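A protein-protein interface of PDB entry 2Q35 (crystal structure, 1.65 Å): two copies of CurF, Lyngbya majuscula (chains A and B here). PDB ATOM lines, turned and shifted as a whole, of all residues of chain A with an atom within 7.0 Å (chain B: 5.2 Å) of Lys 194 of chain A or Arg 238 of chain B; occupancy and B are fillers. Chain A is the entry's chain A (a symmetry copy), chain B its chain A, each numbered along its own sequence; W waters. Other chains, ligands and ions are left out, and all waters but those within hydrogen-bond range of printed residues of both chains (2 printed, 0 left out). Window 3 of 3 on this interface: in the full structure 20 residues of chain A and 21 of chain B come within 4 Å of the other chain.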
ATOM      1  N   ASN A  11       0.481 -21.217   0.296  1.00  0.00           N
ATOM      2  CA  ASN A  11       0.635 -20.662   1.645  1.00  0.00           C
ATOM      3  C   ASN A  11       1.909 -21.113   2.330  1.00  0.00           C
ATOM      4  O   ASN A  11       1.984 -21.121   3.563  1.00  0.00           O
ATOM      5  CB  ASN A  11      -0.577 -21.032   2.491  1.00  0.00           C
ATOM      6  CG  ASN A  11      -1.873 -20.652   1.803  1.00  0.00           C
ATOM      7  OD1 ASN A  11      -1.995 -19.530   1.303  1.00  0.00           O
ATOM      8  ND2 ASN A  11      -2.836 -21.582   1.759  1.00  0.00           N
ATOM      9  N   VAL A  13       3.292 -24.139   2.123  1.00  0.00           N
ATOM     10  CA  VAL A  13       3.373 -25.595   2.331  1.00  0.00           C
ATOM     11  C   VAL A  13       3.903 -26.227   1.044  1.00  0.00           C
ATOM     12  O   VAL A  13       3.419 -25.922  -0.077  1.00  0.00           O
ATOM     13  CB  VAL A  13       1.972 -26.202   2.686  1.00  0.00           C
ATOM     14  CG1 VAL A  13       2.069 -27.682   2.942  1.00  0.00           C
ATOM     15  CG2 VAL A  13       1.416 -25.535   3.925  1.00  0.00           C
ATOM     16  N   LYS A  49       7.313 -22.782   4.491  1.00  0.00           N
ATOM     17  CA  LYS A  49       7.078 -22.851   5.928  1.00  0.00           C
ATOM     18  C   LYS A  49       6.884 -24.266   6.478  1.00  0.00           C
ATOM     19  O   LYS A  49       7.123 -24.495   7.666  1.00  0.00           O
ATOM     20  CB  LYS A  49       5.839 -22.021   6.346  1.00  0.00           C
ATOM     21  CG  LYS A  49       5.926 -20.543   6.100  1.00  0.00           C
ATOM     22  CD  LYS A  49       4.609 -19.982   6.593  1.00  0.00           C
ATOM     23  CE  LYS A  49       4.579 -18.500   6.651  1.00  0.00           C
ATOM     24  NZ  LYS A  49       3.228 -18.083   7.067  1.00  0.00           N
ATOM     25  N   VAL A  50       6.355 -25.178   5.650  1.00  0.00           N
ATOM     26  CA  VAL A  50       6.063 -26.576   6.097  1.00  0.00           C
ATOM     27  C   VAL A  50       6.413 -27.505   4.958  1.00  0.00           C
ATOM     28  O   VAL A  50       6.078 -27.221   3.805  1.00  0.00           O
ATOM     29  CB  VAL A  50       4.554 -26.778   6.494  1.00  0.00           C
ATOM     30  CG1 VAL A  50       4.312 -28.201   6.995  1.00  0.00           C
ATOM     31  CG2 VAL A  50       4.106 -25.785   7.564  1.00  0.00           C
ATOM     32  N   GLY A 189      -0.687 -29.322   7.606  1.00  0.00           N
ATOM     33  CA  GLY A 189       0.383 -28.399   7.154  1.00  0.00           C
ATOM     34  C   GLY A 189      -0.194 -26.998   6.986  1.00  0.00           C
ATOM     35  O   GLY A 189       0.412 -26.010   7.369  1.00  0.00           O
ATOM     36  N   GLN A 190      -1.392 -26.902   6.422  1.00  0.00           N
ATOM     37  CA  GLN A 190      -1.984 -25.581   6.205  1.00  0.00           C
ATOM     38  C   GLN A 190      -2.271 -24.888   7.539  1.00  0.00           C
ATOM     39  O   GLN A 190      -2.131 -23.673   7.643  1.00  0.00           O
ATOM     40  CB  GLN A 190      -3.268 -25.702   5.343  1.00  0.00           C
ATOM     41  CG  GLN A 190      -2.950 -26.086   3.873  1.00  0.00           C
ATOM     42  CD  GLN A 190      -2.156 -25.028   3.087  1.00  0.00           C
ATOM     43  OE1 GLN A 190      -2.163 -23.847   3.421  1.00  0.00           O
ATOM     44  NE2 GLN A 190      -1.492 -25.458   2.032  1.00  0.00           N
ATOM     45  N   LYS A 191      -2.665 -25.654   8.558  1.00  0.00           N
ATOM     46  CA  LYS A 191      -2.899 -25.057   9.883  1.00  0.00           C
ATOM     47  C   LYS A 191      -1.602 -24.513  10.435  1.00  0.00           C
ATOM     48  O   LYS A 191      -1.554 -23.395  10.946  1.00  0.00           O
ATOM     49  CB  LYS A 191      -3.433 -26.078  10.872  1.00  0.00           C
ATOM     50  CG  LYS A 191      -4.861 -26.475  10.620  1.00  0.00           C
ATOM     51  CD  LYS A 191      -5.254 -27.591  11.546  1.00  0.00           C
ATOM     52  CE  LYS A 191      -6.668 -28.078  11.191  1.00  0.00           C
ATOM     53  NZ  LYS A 191      -7.163 -28.985  12.259  1.00  0.00           N
ATOM     54  N   ILE A 192      -0.569 -25.330  10.337  1.00  0.00           N
ATOM     55  CA  ILE A 192       0.754 -24.923  10.860  1.00  0.00           C
ATOM     56  C   ILE A 192       1.246 -23.667  10.137  1.00  0.00           C
ATOM     57  O   ILE A 192       1.786 -22.740  10.783  1.00  0.00           O
ATOM     58  CB  ILE A 192       1.750 -26.071  10.765  1.00  0.00           C
ATOM     59  CG1 ILE A 192       1.330 -27.199  11.712  1.00  0.00           C
ATOM     60  CG2 ILE A 192       3.178 -25.593  11.148  1.00  0.00           C
ATOM     61  CD1 ILE A 192       2.166 -28.489  11.530  1.00  0.00           C
ATOM     62  N   ALA A 193       1.064 -23.634   8.815  1.00  0.00           N
ATOM     63  CA  ALA A 193       1.592 -22.526   7.979  1.00  0.00           C
ATOM     64  C   ALA A 193       0.923 -21.179   8.231  1.00  0.00           C
ATOM     65  O   ALA A 193       1.356 -20.178   7.656  1.00  0.00           O
ATOM     66  CB  ALA A 193       1.550 -22.879   6.483  1.00  0.00           C
ATOM     67  N   LYS A 194      -0.154 -21.146   9.041  1.00  0.00           N
ATOM     68  CA  LYS A 194      -0.786 -19.858   9.402  1.00  0.00           C
ATOM     69  C   LYS A 194       0.129 -18.957  10.249  1.00  0.00           C
ATOM     70  O   LYS A 194      -0.094 -17.742  10.325  1.00  0.00           O
ATOM     71  CB  LYS A 194      -2.130 -20.049  10.117  1.00  0.00           C
ATOM     72  CG  LYS A 194      -3.218 -20.578   9.199  1.00  0.00           C
ATOM     73  CD  LYS A 194      -4.572 -20.611   9.902  1.00  0.00           C
ATOM     74  CE  LYS A 194      -5.632 -21.198   9.004  1.00  0.00           C
ATOM     75  NZ  LYS A 194      -6.944 -21.278   9.713  1.00  0.00           N
ATOM     76  N   SER A 195       1.140 -19.550  10.875  1.00  0.00           N
ATOM     77  CA  SER A 195       2.081 -18.801  11.720  1.00  0.00           C
ATOM     78  C   SER A 195       3.192 -18.172  10.899  1.00  0.00           C
ATOM     79  O   SER A 195       3.546 -18.683   9.834  1.00  0.00           O
ATOM     80  CB  SER A 195       2.717 -19.748  12.725  1.00  0.00           C
ATOM     81  OG  SER A 195       1.768 -20.205  13.668  1.00  0.00           O
ATOM     82  N   PRO A 196       3.784 -17.083  11.413  1.00  0.00           N
ATOM     83  CA  PRO A 196       4.940 -16.470  10.766  1.00  0.00           C
ATOM     84  C   PRO A 196       6.095 -17.464  10.704  1.00  0.00           C
ATOM     85  O   PRO A 196       6.323 -18.237  11.664  1.00  0.00           O
ATOM     86  CB  PRO A 196       5.305 -15.312  11.709  1.00  0.00           C
ATOM     87  CG  PRO A 196       4.036 -15.014  12.497  1.00  0.00           C
ATOM     88  CD  PRO A 196       3.374 -16.360  12.637  1.00  0.00           C
ATOM     89  N   ARG A 197       6.823 -17.439   9.591  1.00  0.00           N
ATOM     90  CA  ARG A 197       7.933 -18.363   9.412  1.00  0.00           C
ATOM     91  C   ARG A 197       8.963 -18.237  10.552  1.00  0.00           C
ATOM     92  O   ARG A 197       9.436 -19.260  11.070  1.00  0.00           O
ATOM     93  CB  ARG A 197       8.615 -18.128   8.062  1.00  0.00           C
ATOM     94  CG  ARG A 197       9.608 -19.205   7.715  1.00  0.00           C
ATOM     95  CD  ARG A 197      10.262 -18.927   6.387  1.00  0.00           C
ATOM     96  NE  ARG A 197      11.202 -19.970   5.975  1.00  0.00           N
ATOM     97  CZ  ARG A 197      12.458 -20.069   6.417  1.00  0.00           C
ATOM     98  NH1 ARG A 197      12.913 -19.239   7.349  1.00  0.00           N
ATOM     99  NH2 ARG A 197      13.231 -21.037   5.963  1.00  0.00           N
ATOM    100  N   LEU A 200       7.827 -20.179  13.490  1.00  0.00           N
ATOM    101  CA  LEU A 200       7.914 -21.636  13.240  1.00  0.00           C
ATOM    102  C   LEU A 200       9.349 -22.145  13.413  1.00  0.00           C
ATOM    103  O   LEU A 200       9.578 -23.174  14.059  1.00  0.00           O
ATOM    104  CB  LEU A 200       7.381 -21.987  11.860  1.00  0.00           C
ATOM    105  CG  LEU A 200       5.861 -21.810  11.697  1.00  0.00           C
ATOM    106  CD1 LEU A 200       5.532 -21.954  10.190  1.00  0.00           C
ATOM    107  CD2 LEU A 200       5.114 -22.813  12.525  1.00  0.00           C
ATOM    108  N   MET B 128       0.725 -19.363  19.415  1.00  0.00           N
ATOM    109  CA  MET B 128       1.061 -19.346  17.991  1.00  0.00           C
ATOM    110  C   MET B 128      -0.098 -18.907  17.092  1.00  0.00           C
ATOM    111  O   MET B 128       0.115 -18.551  15.924  1.00  0.00           O
ATOM    112  CB  MET B 128       1.636 -20.692  17.540  1.00  0.00           C
ATOM    113  CG  MET B 128       3.040 -20.985  18.130  1.00  0.00           C
ATOM    114  SD  MET B 128       4.327 -20.027  17.305  1.00  0.00           S
ATOM    115  CE  MET B 128       4.623 -21.039  15.861  1.00  0.00           C
ATOM    116  N   LYS B 129      -1.307 -18.947  17.639  1.00  0.00           N
ATOM    117  CA  LYS B 129      -2.462 -18.378  16.929  1.00  0.00           C
ATOM    118  C   LYS B 129      -2.258 -16.885  16.726  1.00  0.00           C
ATOM    119  O   LYS B 129      -2.537 -16.352  15.647  1.00  0.00           O
ATOM    120  CB  LYS B 129      -3.756 -18.635  17.681  1.00  0.00           C
ATOM    121  CG  LYS B 129      -4.999 -17.985  17.016  1.00  0.00           C
ATOM    122  CD  LYS B 129      -6.293 -18.734  17.308  1.00  0.00           C
ATOM    123  CE  LYS B 129      -6.632 -19.771  16.219  1.00  0.00           C
ATOM    124  NZ  LYS B 129      -7.821 -20.670  16.543  1.00  0.00           N
ATOM    125  N   TYR B 130      -1.754 -16.208  17.758  1.00  0.00           N
ATOM    126  CA  TYR B 130      -1.381 -14.797  17.640  1.00  0.00           C
ATOM    127  C   TYR B 130      -0.101 -14.600  16.848  1.00  0.00           C
ATOM    128  O   TYR B 130       0.177 -13.494  16.410  1.00  0.00           O
ATOM    129  CB  TYR B 130      -1.153 -14.172  19.010  1.00  0.00           C
ATOM    130  CG  TYR B 130      -2.333 -14.237  19.942  1.00  0.00           C
ATOM    131  CD1 TYR B 130      -3.538 -13.623  19.610  1.00  0.00           C
ATOM    132  CD2 TYR B 130      -2.236 -14.901  21.162  1.00  0.00           C
ATOM    133  CE1 TYR B 130      -4.618 -13.669  20.470  1.00  0.00           C
ATOM    134  CE2 TYR B 130      -3.316 -14.952  22.045  1.00  0.00           C
ATOM    135  CZ  TYR B 130      -4.504 -14.336  21.685  1.00  0.00           C
ATOM    136  OH  TYR B 130      -5.576 -14.383  22.563  1.00  0.00           O
ATOM    137  N   GLY B 131       0.694 -15.661  16.720  1.00  0.00           N
ATOM    138  CA  GLY B 131       1.856 -15.641  15.835  1.00  0.00           C
ATOM    139  C   GLY B 131       3.188 -15.655  16.549  1.00  0.00           C
ATOM    140  O   GLY B 131       4.221 -15.492  15.894  1.00  0.00           O
ATOM    141  N   GLU B 234       4.280  -7.672  12.395  1.00  0.00           N
ATOM    142  CA  GLU B 234       2.920  -8.136  12.058  1.00  0.00           C
ATOM    143  C   GLU B 234       2.098  -8.609  13.253  1.00  0.00           C
ATOM    144  O   GLU B 234       0.891  -8.880  13.127  1.00  0.00           O
ATOM    145  CB  GLU B 234       3.020  -9.284  11.050  1.00  0.00           C
ATOM    146  CG  GLU B 234       3.561 -10.573  11.691  1.00  0.00           C
ATOM    147  CD  GLU B 234       4.313 -11.475  10.736  1.00  0.00           C
ATOM    148  OE1 GLU B 234       3.713 -11.943   9.737  1.00  0.00           O
ATOM    149  OE2 GLU B 234       5.507 -11.735  11.007  1.00  0.00           O
ATOM    150  N   ILE B 235       2.735  -8.735  14.410  1.00  0.00           N
ATOM    151  CA  ILE B 235       2.064  -9.317  15.573  1.00  0.00           C
ATOM    152  C   ILE B 235       0.899  -8.463  16.097  1.00  0.00           C
ATOM    153  O   ILE B 235      -0.157  -9.004  16.420  1.00  0.00           O
ATOM    154  CB  ILE B 235       3.074  -9.664  16.714  1.00  0.00           C
ATOM    155  CG1 ILE B 235       4.072 -10.726  16.235  1.00  0.00           C
ATOM    156  CG2 ILE B 235       2.341 -10.110  18.000  1.00  0.00           C
ATOM    157  CD1 ILE B 235       3.421 -12.057  15.747  1.00  0.00           C
ATOM    158  N   ALA B 236       1.086  -7.146  16.186  1.00  0.00           N
ATOM    159  CA  ALA B 236       0.009  -6.264  16.674  1.00  0.00           C
ATOM    160  C   ALA B 236      -1.281  -6.449  15.871  1.00  0.00           C
ATOM    161  O   ALA B 236      -2.362  -6.544  16.456  1.00  0.00           O
ATOM    162  CB  ALA B 236       0.433  -4.821  16.656  1.00  0.00           C
ATOM    163  N   SER B 237      -1.149  -6.528  14.546  1.00  0.00           N
ATOM    164  CA  SER B 237      -2.303  -6.736  13.663  1.00  0.00           C
ATOM    165  C   SER B 237      -2.953  -8.110  13.852  1.00  0.00           C
ATOM    166  O   SER B 237      -4.190  -8.247  13.811  1.00  0.00           O
ATOM    167  CB  SER B 237      -1.902  -6.521  12.193  1.00  0.00           C
ATOM    168  OG  SER B 237      -2.976  -6.831  11.311  1.00  0.00           O
ATOM    169  N   ARG B 238      -2.126  -9.133  14.059  1.00  0.00           N
ATOM    170  CA  ARG B 238      -2.639 -10.474  14.316  1.00  0.00           C
ATOM    171  C   ARG B 238      -3.460 -10.487  15.606  1.00  0.00           C
ATOM    172  O   ARG B 238      -4.546 -11.083  15.647  1.00  0.00           O
ATOM    173  CB  ARG B 238      -1.490 -11.504  14.361  1.00  0.00           C
ATOM    174  CG  ARG B 238      -0.866 -11.776  13.001  1.00  0.00           C
ATOM    175  CD  ARG B 238       0.270 -12.756  13.122  1.00  0.00           C
ATOM    176  NE  ARG B 238       0.569 -13.458  11.878  1.00  0.00           N
ATOM    177  CZ  ARG B 238       0.257 -14.741  11.627  1.00  0.00           C
ATOM    178  NH1 ARG B 238      -0.350 -15.489  12.541  1.00  0.00           N
ATOM    179  NH2 ARG B 238       0.600 -15.269  10.472  1.00  0.00           N
ATOM    180  N   ILE B 239      -2.963  -9.804  16.646  1.00  0.00           N
ATOM    181  CA  ILE B 239      -3.686  -9.742  17.916  1.00  0.00           C
ATOM    182  C   ILE B 239      -4.995  -8.982  17.700  1.00  0.00           C
ATOM    183  O   ILE B 239      -6.051  -9.430  18.152  1.00  0.00           O
ATOM    184  CB  ILE B 239      -2.863  -9.111  19.056  1.00  0.00           C
ATOM    185  CG1 ILE B 239      -1.608  -9.970  19.310  1.00  0.00           C
ATOM    186  CG2 ILE B 239      -3.721  -8.994  20.339  1.00  0.00           C
ATOM    187  CD1 ILE B 239      -0.507  -9.257  20.082  1.00  0.00           C
ATOM    188  N   GLN B 240      -4.917  -7.853  16.995  1.00  0.00           N
ATOM    189  CA  GLN B 240      -6.127  -7.070  16.673  1.00  0.00           C
ATOM    190  C   GLN B 240      -7.220  -7.939  16.056  1.00  0.00           C
ATOM    191  O   GLN B 240      -8.395  -7.803  16.406  1.00  0.00           O
ATOM    192  CB  GLN B 240      -5.819  -5.912  15.723  1.00  0.00           C
ATOM    193  CG  GLN B 240      -7.092  -5.126  15.314  1.00  0.00           C
ATOM    194  CD  GLN B 240      -6.788  -3.879  14.501  1.00  0.00           C
ATOM    195  OE1 GLN B 240      -5.813  -3.165  14.770  1.00  0.00           O
ATOM    196  NE2 GLN B 240      -7.616  -3.611  13.492  1.00  0.00           N
ATOM    197  N   GLN B 241      -6.836  -8.837  15.153  1.00  0.00           N
ATOM    198  CA  GLN B 241      -7.842  -9.622  14.433  1.00  0.00           C
ATOM    199  C   GLN B 241      -8.427 -10.764  15.258  1.00  0.00           C
ATOM    200  O   GLN B 241      -9.385 -11.394  14.824  1.00  0.00           O
ATOM    201  CB  GLN B 241      -7.305 -10.108  13.084  1.00  0.00           C
ATOM    202  CG  GLN B 241      -6.976  -8.954  12.140  1.00  0.00           C
ATOM    203  CD  GLN B 241      -8.138  -7.966  11.968  1.00  0.00           C
ATOM    204  OE1 GLN B 241      -7.936  -6.745  11.947  1.00  0.00           O
ATOM    205  NE2 GLN B 241      -9.362  -8.496  11.852  1.00  0.00           N
ATOM    206  N   GLU B 242      -7.887 -11.005  16.461  1.00  0.00           N
ATOM    207  CA  GLU B 242      -8.466 -12.035  17.340  1.00  0.00           C
ATOM    208  C   GLU B 242      -9.528 -11.517  18.331  1.00  0.00           C
ATOM    209  O   GLU B 242     -10.135 -12.314  19.057  1.00  0.00           O
ATOM    210  CB  GLU B 242      -7.372 -12.802  18.086  1.00  0.00           C
ATOM    211  CG  GLU B 242      -6.394 -13.576  17.176  1.00  0.00           C
ATOM    212  CD  GLU B 242      -7.080 -14.631  16.311  1.00  0.00           C
ATOM    213  OE1 GLU B 242      -7.806 -15.480  16.871  1.00  0.00           O
ATOM    214  OE2 GLU B 242      -6.883 -14.619  15.072  1.00  0.00           O
HETATM  215  O   HOH W   1      -0.931 -19.281  13.533  1.00  0.00           O
HETATM  216  O   HOH W   2      -2.234 -16.359   9.253  1.00  0.00           O
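The side-chain hydroxyl (OG) of Ser 195 of chain A sits at hydrogen-bond distance from the backbone carbonyl oxygen (O) of Met 128 of chain B (3.2 Å).
The backbone carbonyl oxygen (O) of Lys 194 of chain A is in hydrogen-bond range of the guanidinium group (NH2) of Arg 238 of chain B, at 2.6 Å.
NZ of Lys 49 of chain A is in hydrogen-bond range of O of Ser 195 of chain A (2.8 Å).
NH2 of Arg 238 of chain B touches C of Ser 195 of chain A (3.9 Å).
Pro 196 of chain A touches Gly 131 of chain B (CG to O, 3.4 Å).
Pro 196 of chain A touches Glu 234 of chain B.
Pro 196 of chain A touches Arg 238 of chain B.
Met 128 of chain B touches Leu 200 of chain A.
Of chain B, only Arg 238 comes within 4 Å of Lys 194 of chain A.
Printed residues of chain B within 4 Å of Ser 195 of chain A: Met 128 (3.2 Å) and Arg 238 (3.9 Å).
Of the printed residues of chain A, Gly 131 of chain B touches Pro 196 (3.4 Å).
Of chain A, only Lys 194, Ser 195 and Pro 196 come within 4 Å of Arg 238 of chain B.
The nearest printed residue of chain A that does not touch Gly 131 of chain B is Ser 195 of chain A (5.1 Å).
Printed residues of chain A that touch a printed residue of chain B: Lys 194, Ser 195, Pro 196 and Leu 200.
Hydrophobic or aromatic side chains of chain A that line the printed part of chain B: Pro 196 and Leu 200.
Of the 13 printed residues of chain B, 4 touch a printed residue of chain A.
Printed residues of chain B that touch a printed residue of chain A: Met 128, Gly 131, Glu 234 and Arg 238.
No position is printed for both chains.
Of the 7 pairs that touch across the chains among the printed residues, none has its exchanged pair printed and touching as well.
Water W1 lies within hydrogen-bond range of the backbone carbonyl oxygen of Met 128 of chain B (2.7 Å) and the side-chain hydroxyl of Ser 195 of chain A (2.9 Å).
Water W2 bridges the backbone carbonyl oxygen (O) of Lys 194 of chain A (2.8 Å) and the guanidinium group (NH2) of Arg 238 of chain B (3.3 Å).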
